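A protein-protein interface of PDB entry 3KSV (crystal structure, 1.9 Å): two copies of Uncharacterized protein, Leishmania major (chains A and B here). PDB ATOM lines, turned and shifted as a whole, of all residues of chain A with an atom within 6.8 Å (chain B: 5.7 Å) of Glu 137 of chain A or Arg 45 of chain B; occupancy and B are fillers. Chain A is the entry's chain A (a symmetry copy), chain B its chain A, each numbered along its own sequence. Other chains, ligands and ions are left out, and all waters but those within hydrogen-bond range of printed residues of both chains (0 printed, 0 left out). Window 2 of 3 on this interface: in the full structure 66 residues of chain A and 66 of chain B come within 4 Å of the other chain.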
ATOM      1  N   VAL A 128     -25.662   4.147 -19.690  1.00  0.00           N
ATOM      2  CA  VAL A 128     -24.260   4.483 -19.460  1.00  0.00           C
ATOM      3  C   VAL A 128     -23.621   4.942 -20.773  1.00  0.00           C
ATOM      4  O   VAL A 128     -24.124   4.653 -21.855  1.00  0.00           O
ATOM      5  CB  VAL A 128     -23.492   3.277 -18.879  1.00  0.00           C
ATOM      6  CG1 VAL A 128     -24.098   2.870 -17.545  1.00  0.00           C
ATOM      7  CG2 VAL A 128     -23.520   2.107 -19.832  1.00  0.00           C
ATOM      8  N   LYS A 129     -22.525   5.686 -20.683  1.00  0.00           N
ATOM      9  CA  LYS A 129     -21.819   6.124 -21.885  1.00  0.00           C
ATOM     10  C   LYS A 129     -20.918   4.988 -22.368  1.00  0.00           C
ATOM     11  O   LYS A 129     -20.204   4.362 -21.572  1.00  0.00           O
ATOM     12  CB  LYS A 129     -20.995   7.399 -21.615  1.00  0.00           C
ATOM     13  N   VAL A 130     -20.979   4.696 -23.664  1.00  0.00           N
ATOM     14  CA  VAL A 130     -19.961   3.858 -24.300  1.00  0.00           C
ATOM     15  C   VAL A 130     -19.338   4.638 -25.483  1.00  0.00           C
ATOM     16  O   VAL A 130     -20.023   5.391 -26.193  1.00  0.00           O
ATOM     17  CB  VAL A 130     -20.499   2.444 -24.726  1.00  0.00           C
ATOM     18  CG1 VAL A 130     -19.423   1.651 -25.443  1.00  0.00           C
ATOM     19  CG2 VAL A 130     -20.974   1.640 -23.506  1.00  0.00           C
ATOM     20  N   ALA A 131     -18.035   4.443 -25.677  1.00  0.00           N
ATOM     21  CA  ALA A 131     -17.278   5.154 -26.688  1.00  0.00           C
ATOM     22  C   ALA A 131     -17.443   4.477 -28.042  1.00  0.00           C
ATOM     23  O   ALA A 131     -17.772   3.301 -28.105  1.00  0.00           O
ATOM     24  CB  ALA A 131     -15.812   5.185 -26.277  1.00  0.00           C
ATOM     25  N   SER A 132     -17.185   5.224 -29.116  1.00  0.00           N
ATOM     26  CA  SER A 132     -17.216   4.678 -30.471  1.00  0.00           C
ATOM     27  C   SER A 132     -16.239   3.521 -30.632  1.00  0.00           C
ATOM     28  O   SER A 132     -16.591   2.483 -31.207  1.00  0.00           O
ATOM     29  CB  SER A 132     -16.922   5.766 -31.520  1.00  0.00           C
ATOM     30  OG  SER A 132     -15.547   6.126 -31.556  1.00  0.00           O
ATOM     31  N   ASP A 133     -15.018   3.685 -30.125  1.00  0.00           N
ATOM     32  CA  ASP A 133     -14.012   2.598 -30.182  1.00  0.00           C
ATOM     33  C   ASP A 133     -14.491   1.295 -29.492  1.00  0.00           C
ATOM     34  O   ASP A 133     -14.297   0.199 -30.013  1.00  0.00           O
ATOM     35  CB  ASP A 133     -12.633   3.047 -29.648  1.00  0.00           C
ATOM     36  CG  ASP A 133     -12.651   3.446 -28.166  1.00  0.00           C
ATOM     37  OD1 ASP A 133     -13.726   3.762 -27.625  1.00  0.00           O
ATOM     38  OD2 ASP A 133     -11.566   3.460 -27.538  1.00  0.00           O
ATOM     39  N   GLU A 134     -15.144   1.429 -28.348  1.00  0.00           N
ATOM     40  CA  GLU A 134     -15.681   0.274 -27.617  1.00  0.00           C
ATOM     41  C   GLU A 134     -16.830  -0.407 -28.360  1.00  0.00           C
ATOM     42  O   GLU A 134     -16.945  -1.632 -28.354  1.00  0.00           O
ATOM     43  CB  GLU A 134     -16.129   0.706 -26.219  1.00  0.00           C
ATOM     44  CG  GLU A 134     -14.968   1.147 -25.333  1.00  0.00           C
ATOM     45  CD  GLU A 134     -15.407   1.790 -24.029  1.00  0.00           C
ATOM     46  OE1 GLU A 134     -16.586   2.207 -23.891  1.00  0.00           O
ATOM     47  OE2 GLU A 134     -14.536   1.909 -23.136  1.00  0.00           O
ATOM     48  N   LEU A 135     -17.686   0.389 -28.996  1.00  0.00           N
ATOM     49  CA  LEU A 135     -18.784  -0.133 -29.787  1.00  0.00           C
ATOM     50  C   LEU A 135     -18.269  -0.938 -30.965  1.00  0.00           C
ATOM     51  O   LEU A 135     -18.887  -1.933 -31.338  1.00  0.00           O
ATOM     52  CB  LEU A 135     -19.660   1.009 -30.326  1.00  0.00           C
ATOM     53  CG  LEU A 135     -20.643   1.641 -29.350  1.00  0.00           C
ATOM     54  CD1 LEU A 135     -21.348   2.823 -30.040  1.00  0.00           C
ATOM     55  CD2 LEU A 135     -21.651   0.607 -28.846  1.00  0.00           C
ATOM     56  N   ALA A 136     -17.175  -0.491 -31.574  1.00  0.00           N
ATOM     57  CA  ALA A 136     -16.644  -1.171 -32.754  1.00  0.00           C
ATOM     58  C   ALA A 136     -16.045  -2.530 -32.367  1.00  0.00           C
ATOM     59  O   ALA A 136     -16.205  -3.538 -33.059  1.00  0.00           O
ATOM     60  CB  ALA A 136     -15.583  -0.294 -33.419  1.00  0.00           C
ATOM     61  N   GLU A 137     -15.330  -2.509 -31.253  1.00  0.00           N
ATOM     62  CA  GLU A 137     -14.731  -3.677 -30.643  1.00  0.00           C
ATOM     63  C   GLU A 137     -15.793  -4.742 -30.314  1.00  0.00           C
ATOM     64  O   GLU A 137     -15.693  -5.896 -30.730  1.00  0.00           O
ATOM     65  CB  GLU A 137     -13.996  -3.181 -29.396  1.00  0.00           C
ATOM     66  CG  GLU A 137     -13.201  -4.184 -28.638  1.00  0.00           C
ATOM     67  CD  GLU A 137     -12.194  -3.507 -27.711  1.00  0.00           C
ATOM     68  OE1 GLU A 137     -12.535  -2.478 -27.051  1.00  0.00           O
ATOM     69  OE2 GLU A 137     -11.057  -4.013 -27.662  1.00  0.00           O
ATOM     70  N   ASP A 138     -16.848  -4.335 -29.624  1.00  0.00           N
ATOM     71  CA  ASP A 138     -17.945  -5.250 -29.316  1.00  0.00           C
ATOM     72  C   ASP A 138     -18.633  -5.734 -30.591  1.00  0.00           C
ATOM     73  O   ASP A 138     -18.999  -6.892 -30.674  1.00  0.00           O
ATOM     74  CB  ASP A 138     -18.984  -4.604 -28.384  1.00  0.00           C
ATOM     75  CG  ASP A 138     -18.395  -4.168 -27.042  1.00  0.00           C
ATOM     76  OD1 ASP A 138     -17.265  -4.596 -26.685  1.00  0.00           O
ATOM     77  OD2 ASP A 138     -19.070  -3.377 -26.342  1.00  0.00           O
ATOM     78  N   ALA A 139     -18.809  -4.857 -31.584  1.00  0.00           N
ATOM     79  CA  ALA A 139     -19.522  -5.240 -32.811  1.00  0.00           C
ATOM     80  C   ALA A 139     -18.738  -6.288 -33.573  1.00  0.00           C
ATOM     81  O   ALA A 139     -19.317  -7.221 -34.120  1.00  0.00           O
ATOM     82  CB  ALA A 139     -19.778  -4.023 -33.694  1.00  0.00           C
ATOM     83  N   LYS A 140     -17.411  -6.127 -33.604  1.00  0.00           N
ATOM     84  CA  LYS A 140     -16.530  -7.079 -34.261  1.00  0.00           C
ATOM     85  C   LYS A 140     -16.552  -8.445 -33.576  1.00  0.00           C
ATOM     86  O   LYS A 140     -16.691  -9.475 -34.234  1.00  0.00           O
ATOM     87  CB  LYS A 140     -15.090  -6.564 -34.276  1.00  0.00           C
ATOM     88  CG  LYS A 140     -14.095  -7.525 -34.941  1.00  0.00           C
ATOM     89  CD  LYS A 140     -12.662  -6.952 -34.935  1.00  0.00           C
ATOM     90  CE  LYS A 140     -11.632  -7.925 -35.527  1.00  0.00           C
ATOM     91  NZ  LYS A 140     -10.245  -7.561 -35.092  1.00  0.00           N
ATOM     92  N   ARG A 141     -16.377  -8.439 -32.259  1.00  0.00           N
ATOM     93  CA  ARG A 141     -16.355  -9.687 -31.468  1.00  0.00           C
ATOM     94  C   ARG A 141     -17.688 -10.440 -31.622  1.00  0.00           C
ATOM     95  O   ARG A 141     -17.722 -11.622 -31.936  1.00  0.00           O
ATOM     96  CB  ARG A 141     -16.095  -9.369 -29.991  1.00  0.00           C
ATOM     97  CG  ARG A 141     -16.226 -10.590 -29.045  1.00  0.00           C
ATOM     98  CD  ARG A 141     -15.495 -10.371 -27.728  1.00  0.00           C
ATOM     99  NE  ARG A 141     -16.152  -9.386 -26.865  1.00  0.00           N
ATOM    100  CZ  ARG A 141     -17.216  -9.616 -26.102  1.00  0.00           C
ATOM    101  NH1 ARG A 141     -17.839 -10.814 -26.101  1.00  0.00           N
ATOM    102  NH2 ARG A 141     -17.695  -8.627 -25.345  1.00  0.00           N
ATOM    103  N   TYR A 142     -18.782  -9.731 -31.425  1.00  0.00           N
ATOM    104  CA  TYR A 142     -20.109 -10.316 -31.582  1.00  0.00           C
ATOM    105  C   TYR A 142     -20.376 -10.862 -32.996  1.00  0.00           C
ATOM    106  O   TYR A 142     -20.899 -11.968 -33.147  1.00  0.00           O
ATOM    107  CB  TYR A 142     -21.171  -9.270 -31.254  1.00  0.00           C
ATOM    108  CG  TYR A 142     -21.393  -8.953 -29.788  1.00  0.00           C
ATOM    109  CD1 TYR A 142     -20.656  -9.562 -28.766  1.00  0.00           C
ATOM    110  CD2 TYR A 142     -22.362  -8.030 -29.433  1.00  0.00           C
ATOM    111  CE1 TYR A 142     -20.898  -9.251 -27.440  1.00  0.00           C
ATOM    112  CE2 TYR A 142     -22.614  -7.719 -28.116  1.00  0.00           C
ATOM    113  CZ  TYR A 142     -21.883  -8.320 -27.130  1.00  0.00           C
ATOM    114  OH  TYR A 142     -22.161  -7.969 -25.847  1.00  0.00           O
ATOM    115  N   PRO B  42     -26.754   2.251 -24.193  1.00  0.00           N
ATOM    116  CA  PRO B  42     -26.762   0.983 -23.466  1.00  0.00           C
ATOM    117  C   PRO B  42     -26.993   1.134 -21.971  1.00  0.00           C
ATOM    118  O   PRO B  42     -26.640   2.165 -21.412  1.00  0.00           O
ATOM    119  CB  PRO B  42     -25.342   0.469 -23.692  1.00  0.00           C
ATOM    120  CG  PRO B  42     -24.522   1.689 -23.766  1.00  0.00           C
ATOM    121  CD  PRO B  42     -25.374   2.678 -24.504  1.00  0.00           C
ATOM    122  N   LEU B  43     -27.534   0.094 -21.329  1.00  0.00           N
ATOM    123  CA  LEU B  43     -27.623   0.016 -19.868  1.00  0.00           C
ATOM    124  C   LEU B  43     -26.361  -0.584 -19.268  1.00  0.00           C
ATOM    125  O   LEU B  43     -26.117  -0.470 -18.065  1.00  0.00           O
ATOM    126  CB  LEU B  43     -28.792  -0.863 -19.443  1.00  0.00           C
ATOM    127  CG  LEU B  43     -30.207  -0.459 -19.836  1.00  0.00           C
ATOM    128  CD1 LEU B  43     -31.142  -1.455 -19.198  1.00  0.00           C
ATOM    129  CD2 LEU B  43     -30.552   0.966 -19.440  1.00  0.00           C
ATOM    130  N   SER B  44     -25.589  -1.251 -20.120  1.00  0.00           N
ATOM    131  CA  SER B  44     -24.347  -1.900 -19.733  1.00  0.00           C
ATOM    132  C   SER B  44     -23.511  -2.070 -20.994  1.00  0.00           C
ATOM    133  O   SER B  44     -24.026  -1.994 -22.114  1.00  0.00           O
ATOM    134  CB  SER B  44     -24.640  -3.259 -19.110  1.00  0.00           C
ATOM    135  OG  SER B  44     -25.343  -4.069 -20.033  1.00  0.00           O
ATOM    136  N   ARG B  45     -22.218  -2.275 -20.809  1.00  0.00           N
ATOM    137  CA  ARG B  45     -21.290  -2.500 -21.910  1.00  0.00           C
ATOM    138  C   ARG B  45     -21.640  -3.804 -22.655  1.00  0.00           C
ATOM    139  O   ARG B  45     -21.789  -4.851 -22.029  1.00  0.00           O
ATOM    140  CB  ARG B  45     -19.861  -2.536 -21.331  1.00  0.00           C
ATOM    141  CG  ARG B  45     -18.747  -2.863 -22.303  1.00  0.00           C
ATOM    142  CD  ARG B  45     -18.494  -1.776 -23.316  1.00  0.00           C
ATOM    143  NE  ARG B  45     -17.580  -2.283 -24.338  1.00  0.00           N
ATOM    144  CZ  ARG B  45     -16.243  -2.305 -24.260  1.00  0.00           C
ATOM    145  NH1 ARG B  45     -15.582  -1.800 -23.211  1.00  0.00           N
ATOM    146  NH2 ARG B  45     -15.553  -2.817 -25.280  1.00  0.00           N
ATOM    147  N   GLY B  46     -21.797  -3.724 -23.982  1.00  0.00           N
ATOM    148  CA  GLY B  46     -22.142  -4.892 -24.829  1.00  0.00           C
ATOM    149  C   GLY B  46     -23.633  -5.122 -25.085  1.00  0.00           C
ATOM    150  O   GLY B  46     -24.016  -6.122 -25.685  1.00  0.00           O
ATOM    151  N   HIS B  47     -24.467  -4.212 -24.581  1.00  0.00           N
ATOM    152  CA  HIS B  47     -25.920  -4.178 -24.822  1.00  0.00           C
ATOM    153  C   HIS B  47     -26.201  -4.072 -26.316  1.00  0.00           C
ATOM    154  O   HIS B  47     -25.722  -3.147 -26.999  1.00  0.00           O
ATOM    155  CB  HIS B  47     -26.515  -2.975 -24.064  1.00  0.00           C
ATOM    156  CG  HIS B  47     -28.009  -2.800 -24.178  1.00  0.00           C
ATOM    157  ND1 HIS B  47     -28.694  -1.911 -23.376  1.00  0.00           N
ATOM    158  CD2 HIS B  47     -28.939  -3.358 -24.995  1.00  0.00           C
ATOM    159  CE1 HIS B  47     -29.977  -1.935 -23.684  1.00  0.00           C
ATOM    160  NE2 HIS B  47     -30.154  -2.805 -24.663  1.00  0.00           N
ATOM    161  N   PRO B 113     -26.143  -7.298 -21.116  1.00  0.00           N
ATOM    162  CA  PRO B 113     -25.201  -7.924 -20.182  1.00  0.00           C
ATOM    163  C   PRO B 113     -25.448  -7.463 -18.761  1.00  0.00           C
ATOM    164  O   PRO B 113     -25.737  -6.281 -18.540  1.00  0.00           O
ATOM    165  CB  PRO B 113     -23.836  -7.419 -20.653  1.00  0.00           C
ATOM    166  CG  PRO B 113     -24.043  -7.142 -22.118  1.00  0.00           C
ATOM    167  CD  PRO B 113     -25.445  -6.671 -22.253  1.00  0.00           C
ATOM    168  N   THR B 115     -23.339  -7.420 -15.753  1.00  0.00           N
ATOM    169  CA  THR B 115     -21.986  -7.575 -15.284  1.00  0.00           C
ATOM    170  C   THR B 115     -21.979  -7.389 -13.774  1.00  0.00           C
ATOM    171  O   THR B 115     -21.126  -7.914 -13.085  1.00  0.00           O
ATOM    172  CB  THR B 115     -21.014  -6.612 -16.055  1.00  0.00           C
ATOM    173  OG1 THR B 115     -19.901  -6.295 -15.229  1.00  0.00           O
ATOM    174  CG2 THR B 115     -21.694  -5.300 -16.516  1.00  0.00           C
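The backbone carbonyl oxygen (O) of Pro 42 of chain B is in hydrogen-bond range of the backbone NH (N) of Val 128 of chain A, 2.8 Å away. The guanidinium group (NH1) of Arg 45 of chain B is in salt-bridge range of the side-chain carboxylate (OE2) of Glu 134 of chain A. The side-chain carboxylate of Glu 137 of chain A is in salt-bridge range of the guanidinium group of Arg 45 of chain B. The side-chain carboxylate (OD2) of Asp 138 of chain A lies within salt-bridge range of the guanidinium group (NE) of Arg 45 of chain B. O of Gly 46 of chain B lies within hydrogen-bond range of OH of Tyr 142 of chain A (2.6 Å).
ND1 of His 47 of chain B sits at hydrogen-bond distance from N of Leu 43 of chain B (3.1 Å). OG of Ser 44 of chain B lies within hydrogen-bond range of O of Pro 113 of chain B (2.7 Å). The backbone NH (N) of Ala 131 of chain A lies within hydrogen-bond range of the side-chain carboxylate (OE1) of Glu 134 of chain A.
CG1 of Val 128 of chain A touches O of Leu 43 of chain B, at 3.9 Å. N of Ser 44 of chain B touches CG2 of Val 128 of chain A, at 3.95 Å. Pro 42 of chain B touches Val 130 of chain A (CG to CG2, 3.6 Å). OD2 of Asp 138 of chain A touches N of Gly 46 of chain B (3.6 Å).
Glu 137 of chain A touches just one residue of chain B: Arg 45. Arg 45 of chain B touches three residues of chain A. Printed residues of chain A within 4 Å of Ser 44 of chain B: Val 128. Of the printed residues of chain B, Tyr 142 of chain A touches Gly 46. Printed residues of chain B within 4 Å of Val 128 of chain A: Pro 42, Leu 43 and Ser 44. Of the printed residues of chain B, Asp 138 of chain A touches Arg 45 and Gly 46. The nearest printed residue of chain B that does not touch Glu 137 of chain A is Gly 46 of chain B (8.4 Å). The nearest residue of chain A that does not touch Arg 45 of chain B is Val 130 of chain A (4.1 Å). The nearest printed residue of chain B that does not touch Asp 138 of chain A is His 47 of chain B (5.7 Å).
Hydrophobic or aromatic side chains of chain A that line the printed part of chain B: Val 128, Val 130 and Tyr 142. Along chain A the printed residues that touch a printed residue of chain B span positions 128 to 142. Hydrophobic or aromatic side chains of chain B within 4 Å of the printed part of chain A: Pro 42. Among the printed residues, 9 pairs touch across the chains. Among the printed residues, Asp or Glu carboxylates within 4 Å of a Lys or Arg side-chain nitrogen of the other chain: Glu 134 of chain A with Arg 45 of chain B (3.9 Å), Glu 137 of chain A with Arg 45 of chain B (3.5 Å) and Asp 138 of chain A with Arg 45 of chain B (2.7 Å).
No position is printed for both chains.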
